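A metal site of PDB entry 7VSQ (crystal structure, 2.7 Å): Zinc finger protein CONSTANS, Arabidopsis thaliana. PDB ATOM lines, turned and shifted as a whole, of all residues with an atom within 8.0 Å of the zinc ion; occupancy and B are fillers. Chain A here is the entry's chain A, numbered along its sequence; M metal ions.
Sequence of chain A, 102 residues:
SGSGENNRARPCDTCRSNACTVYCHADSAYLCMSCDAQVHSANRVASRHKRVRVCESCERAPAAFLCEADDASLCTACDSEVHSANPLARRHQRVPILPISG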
ATOM      1  N   LEU A  66       3.283 -15.491  34.200  1.00  0.00           N
ATOM      2  CA  LEU A  66       3.027 -14.087  34.541  1.00  0.00           C
ATOM      3  C   LEU A  66       3.888 -13.177  33.645  1.00  0.00           C
ATOM      4  O   LEU A  66       5.030 -13.518  33.324  1.00  0.00           O
ATOM      5  CB  LEU A  66       3.365 -13.820  36.014  1.00  0.00           C
ATOM      6  CG  LEU A  66       3.246 -12.374  36.509  1.00  0.00           C
ATOM      7  CD1 LEU A  66       1.897 -11.768  36.152  1.00  0.00           C
ATOM      8  CD2 LEU A  66       3.541 -12.248  37.997  1.00  0.00           C
ATOM      9  N   CYS A  67       3.340 -12.044  33.243  1.00  0.00           N
ATOM     10  CA  CYS A  67       4.122 -11.000  32.596  1.00  0.00           C
ATOM     11  C   CYS A  67       3.889  -9.696  33.342  1.00  0.00           C
ATOM     12  O   CYS A  67       2.746  -9.319  33.606  1.00  0.00           O
ATOM     13  CB  CYS A  67       3.734 -10.849  31.125  1.00  0.00           C
ATOM     14  SG  CYS A  67       4.761  -9.670  30.215  1.00  0.00           S
ATOM     15  N   GLU A  68       4.976  -8.988  33.630  1.00  0.00           N
ATOM     16  CA  GLU A  68       4.910  -7.697  34.294  1.00  0.00           C
ATOM     17  C   GLU A  68       4.551  -6.606  33.305  1.00  0.00           C
ATOM     18  O   GLU A  68       3.803  -5.678  33.623  1.00  0.00           O
ATOM     19  CB  GLU A  68       6.252  -7.352  34.954  1.00  0.00           C
ATOM     20  CG  GLU A  68       6.247  -7.276  36.474  1.00  0.00           C
ATOM     21  CD  GLU A  68       7.652  -7.090  37.039  1.00  0.00           C
ATOM     22  OE1 GLU A  68       8.565  -6.733  36.265  1.00  0.00           O
ATOM     23  OE2 GLU A  68       7.840  -7.298  38.251  1.00  0.00           O
ATOM     24  N   ALA A  69       5.096  -6.726  32.109  1.00  0.00           N
ATOM     25  CA  ALA A  69       4.882  -5.745  31.050  1.00  0.00           C
ATOM     26  C   ALA A  69       3.442  -5.841  30.561  1.00  0.00           C
ATOM     27  O   ALA A  69       2.787  -4.832  30.342  1.00  0.00           O
ATOM     28  CB  ALA A  69       5.860  -5.945  29.937  1.00  0.00           C
ATOM     29  N   ASP A  70       2.946  -7.062  30.370  1.00  0.00           N
ATOM     30  CA  ASP A  70       1.565  -7.257  29.949  1.00  0.00           C
ATOM     31  C   ASP A  70       0.619  -7.177  31.153  1.00  0.00           C
ATOM     32  O   ASP A  70      -0.598  -7.135  30.979  1.00  0.00           O
ATOM     33  CB  ASP A  70       1.389  -8.590  29.228  1.00  0.00           C
ATOM     34  CG  ASP A  70       2.112  -8.643  27.892  1.00  0.00           C
ATOM     35  OD1 ASP A  70       2.624  -9.721  27.533  1.00  0.00           O
ATOM     36  OD2 ASP A  70       2.171  -7.604  27.191  1.00  0.00           O
ATOM     37  N   ASP A  71       1.202  -7.117  32.352  1.00  0.00           N
ATOM     38  CA  ASP A  71       0.473  -7.266  33.621  1.00  0.00           C
ATOM     39  C   ASP A  71      -0.609  -8.338  33.464  1.00  0.00           C
ATOM     40  O   ASP A  71      -1.796  -8.100  33.708  1.00  0.00           O
ATOM     41  CB  ASP A  71      -0.122  -5.900  34.036  1.00  0.00           C
ATOM     42  CG  ASP A  71      -0.959  -5.969  35.322  1.00  0.00           C
ATOM     43  OD1 ASP A  71      -0.690  -6.858  36.162  1.00  0.00           O
ATOM     44  OD2 ASP A  71      -1.865  -5.124  35.476  1.00  0.00           O
ATOM     45  N   ALA A  72      -0.181  -9.530  33.049  1.00  0.00           N
ATOM     46  CA  ALA A  72      -1.153 -10.618  32.885  1.00  0.00           C
ATOM     47  C   ALA A  72      -0.627 -12.039  33.131  1.00  0.00           C
ATOM     48  O   ALA A  72       0.539 -12.325  32.905  1.00  0.00           O
ATOM     49  CB  ALA A  72      -1.761 -10.547  31.495  1.00  0.00           C
ATOM     50  N   LEU A  74      -1.172 -15.972  31.940  1.00  0.00           N
ATOM     51  CA  LEU A  74      -1.660 -16.667  30.746  1.00  0.00           C
ATOM     52  C   LEU A  74      -1.267 -18.145  30.674  1.00  0.00           C
ATOM     53  O   LEU A  74      -0.294 -18.573  31.316  1.00  0.00           O
ATOM     54  CB  LEU A  74      -1.127 -15.969  29.503  1.00  0.00           C
ATOM     55  CG  LEU A  74      -1.089 -14.456  29.558  1.00  0.00           C
ATOM     56  CD1 LEU A  74      -0.153 -13.899  28.493  1.00  0.00           C
ATOM     57  CD2 LEU A  74      -2.482 -13.880  29.406  1.00  0.00           C
ATOM     58  N   ASP A  79       0.115 -17.686  26.366  1.00  0.00           N
ATOM     59  CA  ASP A  79       1.353 -16.992  26.689  1.00  0.00           C
ATOM     60  C   ASP A  79       2.233 -16.924  25.460  1.00  0.00           C
ATOM     61  O   ASP A  79       2.796 -15.877  25.135  1.00  0.00           O
ATOM     62  CB  ASP A  79       2.088 -17.691  27.837  1.00  0.00           C
ATOM     63  CG  ASP A  79       3.452 -17.120  28.109  1.00  0.00           C
ATOM     64  OD1 ASP A  79       4.430 -17.580  27.484  1.00  0.00           O
ATOM     65  OD2 ASP A  79       3.523 -16.202  28.949  1.00  0.00           O
ATOM     66  N   VAL A  82       0.517 -14.587  22.629  1.00  0.00           N
ATOM     67  CA  VAL A  82       0.588 -13.133  22.821  1.00  0.00           C
ATOM     68  C   VAL A  82       1.946 -12.602  22.388  1.00  0.00           C
ATOM     69  O   VAL A  82       2.039 -11.552  21.748  1.00  0.00           O
ATOM     70  CB  VAL A  82       0.308 -12.736  24.294  1.00  0.00           C
ATOM     71  CG1 VAL A  82       0.822 -11.347  24.595  1.00  0.00           C
ATOM     72  CG2 VAL A  82      -1.185 -12.807  24.582  1.00  0.00           C
ATOM     73  N   HIS A  83       2.991 -13.335  22.706  1.00  0.00           N
ATOM     74  CA  HIS A  83       4.344 -12.883  22.435  1.00  0.00           C
ATOM     75  C   HIS A  83       4.925 -13.463  21.146  1.00  0.00           C
ATOM     76  O   HIS A  83       6.090 -13.265  20.835  1.00  0.00           O
ATOM     77  CB  HIS A  83       5.230 -13.178  23.641  1.00  0.00           C
ATOM     78  CG  HIS A  83       4.646 -12.679  24.931  1.00  0.00           C
ATOM     79  ND1 HIS A  83       3.612 -13.328  25.579  1.00  0.00           N
ATOM     80  CD2 HIS A  83       4.907 -11.576  25.654  1.00  0.00           C
ATOM     81  CE1 HIS A  83       3.286 -12.651  26.660  1.00  0.00           C
ATOM     82  NE2 HIS A  83       4.054 -11.578  26.739  1.00  0.00           N
ATOM     83  N   LEU A  88       8.627  -7.238  19.215  1.00  0.00           N
ATOM     84  CA  LEU A  88       8.357  -6.405  20.365  1.00  0.00           C
ATOM     85  C   LEU A  88       7.767  -7.215  21.514  1.00  0.00           C
ATOM     86  O   LEU A  88       8.229  -7.147  22.645  1.00  0.00           O
ATOM     87  CB  LEU A  88       7.407  -5.296  19.938  1.00  0.00           C
ATOM     88  CG  LEU A  88       7.493  -3.953  20.634  1.00  0.00           C
ATOM     89  CD1 LEU A  88       6.766  -2.944  19.781  1.00  0.00           C
ATOM     90  CD2 LEU A  88       6.846  -4.073  21.975  1.00  0.00           C
ATOM     91  N   ALA A  89       6.707  -7.957  21.187  1.00  0.00           N
ATOM     92  CA  ALA A  89       6.012  -8.785  22.167  1.00  0.00           C
ATOM     93  C   ALA A  89       6.881  -9.944  22.626  1.00  0.00           C
ATOM     94  O   ALA A  89       6.863 -10.330  23.790  1.00  0.00           O
ATOM     95  CB  ALA A  89       4.708  -9.289  21.574  1.00  0.00           C
ATOM     96  N   ARG A  90       7.647 -10.491  21.691  1.00  0.00           N
ATOM     97  CA  ARG A  90       8.541 -11.607  21.985  1.00  0.00           C
ATOM     98  C   ARG A  90       9.588 -11.230  23.035  1.00  0.00           C
ATOM     99  O   ARG A  90      10.006 -12.075  23.831  1.00  0.00           O
ATOM    100  CB  ARG A  90       9.216 -12.069  20.681  1.00  0.00           C
ATOM    101  CG  ARG A  90      10.631 -12.524  20.819  1.00  0.00           C
ATOM    102  CD  ARG A  90      11.142 -13.225  19.581  1.00  0.00           C
ATOM    103  NE  ARG A  90      12.511 -13.674  19.811  1.00  0.00           N
ATOM    104  CZ  ARG A  90      12.815 -14.812  20.401  1.00  0.00           C
ATOM    105  NH1 ARG A  90      11.859 -15.640  20.803  1.00  0.00           N
ATOM    106  NH2 ARG A  90      14.084 -15.141  20.578  1.00  0.00           N
ATOM    107  N   ARG A  91       9.979  -9.972  23.071  1.00  0.00           N
ATOM    108  CA  ARG A  91      11.032  -9.541  23.973  1.00  0.00           C
ATOM    109  C   ARG A  91      10.574  -9.478  25.430  1.00  0.00           C
ATOM    110  O   ARG A  91      11.406  -9.490  26.347  1.00  0.00           O
ATOM    111  CB  ARG A  91      11.577  -8.190  23.495  1.00  0.00           C
ATOM    112  CG  ARG A  91      12.284  -7.310  24.512  1.00  0.00           C
ATOM    113  CD  ARG A  91      12.995  -6.193  23.792  1.00  0.00           C
ATOM    114  NE  ARG A  91      12.057  -5.375  23.025  1.00  0.00           N
ATOM    115  CZ  ARG A  91      12.406  -4.473  22.112  1.00  0.00           C
ATOM    116  NH1 ARG A  91      13.682  -4.272  21.828  1.00  0.00           N
ATOM    117  NH2 ARG A  91      11.479  -3.782  21.465  1.00  0.00           N
ATOM    118  N   HIS A  92       9.269  -9.508  25.650  1.00  0.00           N
ATOM    119  CA  HIS A  92       8.706  -9.516  27.003  1.00  0.00           C
ATOM    120  C   HIS A  92       9.267 -10.674  27.800  1.00  0.00           C
ATOM    121  O   HIS A  92       9.344 -11.797  27.304  1.00  0.00           O
ATOM    122  CB  HIS A  92       7.181  -9.620  26.975  1.00  0.00           C
ATOM    123  CG  HIS A  92       6.503  -8.481  26.286  1.00  0.00           C
ATOM    124  ND1 HIS A  92       5.342  -7.910  26.763  1.00  0.00           N
ATOM    125  CD2 HIS A  92       6.809  -7.812  25.152  1.00  0.00           C
ATOM    126  CE1 HIS A  92       4.966  -6.937  25.948  1.00  0.00           C
ATOM    127  NE2 HIS A  92       5.844  -6.867  24.961  1.00  0.00           N
ATOM    128  N   GLN A  93       9.667 -10.405  29.038  1.00  0.00           N
ATOM    129  CA  GLN A  93      10.173 -11.468  29.899  1.00  0.00           C
ATOM    130  C   GLN A  93       9.093 -11.984  30.854  1.00  0.00           C
ATOM    131  O   GLN A  93       8.630 -11.275  31.750  1.00  0.00           O
ATOM    132  CB  GLN A  93      11.402 -11.030  30.696  1.00  0.00           C
ATOM    133  CG  GLN A  93      12.640 -10.747  29.857  1.00  0.00           C
ATOM    134  CD  GLN A  93      13.735 -10.043  30.633  1.00  0.00           C
ATOM    135  OE1 GLN A  93      13.476  -9.407  31.665  1.00  0.00           O
ATOM    136  NE2 GLN A  93      14.977 -10.227  30.205  1.00  0.00           N
ATOM    137  N   ARG A  94       8.675 -13.220  30.598  1.00  0.00           N
ATOM    138  CA  ARG A  94       7.605 -13.848  31.341  1.00  0.00           C
ATOM    139  C   ARG A  94       8.166 -14.864  32.323  1.00  0.00           C
ATOM    140  O   ARG A  94       9.257 -15.393  32.115  1.00  0.00           O
ATOM    141  CB  ARG A  94       6.644 -14.518  30.365  1.00  0.00           C
ATOM    142  CG  ARG A  94       6.039 -13.590  29.333  1.00  0.00           C
ATOM    143  CD  ARG A  94       5.727 -14.339  28.046  1.00  0.00           C
ATOM    144  NE  ARG A  94       6.922 -14.783  27.331  1.00  0.00           N
ATOM    145  CZ  ARG A  94       6.938 -15.760  26.429  1.00  0.00           C
ATOM    146  NH1 ARG A  94       8.060 -16.092  25.826  1.00  0.00           N
ATOM    147  NH2 ARG A  94       5.821 -16.423  26.140  1.00  0.00           N
HETATM  148 ZN    ZN M   1       4.345 -10.023  27.997  1.00  0.00          ZN
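OD2 of Asp 70 sits close to ND1 of His 92, at 3.2 Å. The backbone carbonyl oxygen of Asp 79 is in hydrogen-bond range of a ring nitrogen (ND1) of His 83, 2.7 Å away. O of His 83 sits close to N of Arg 90 (3.3 Å). SG of Cys 67 sits close to N of Ala 69 (3.5 Å). The backbone NH of Cys 67 sits at hydrogen-bond distance from the backbone carbonyl oxygen of Ala 72. The backbone carbonyl oxygen (O) of Leu 88 lies close to a ring nitrogen (NE2) of His 92.
Of the 18 residues printed, 4 come within 4 Å of the zinc ion. The nearest printed residue that does not touch the zinc ion is Arg 94 (4.2 Å).
OD1 of Asp 70 binds the zinc ion. NE2 of His 83 binds the zinc ion. SG of Cys 67 binds the zinc ion, at 2.3 Å. Slightly farther from the zinc ion lies a ring nitrogen (ND1) of His 92 (2.6 Å).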
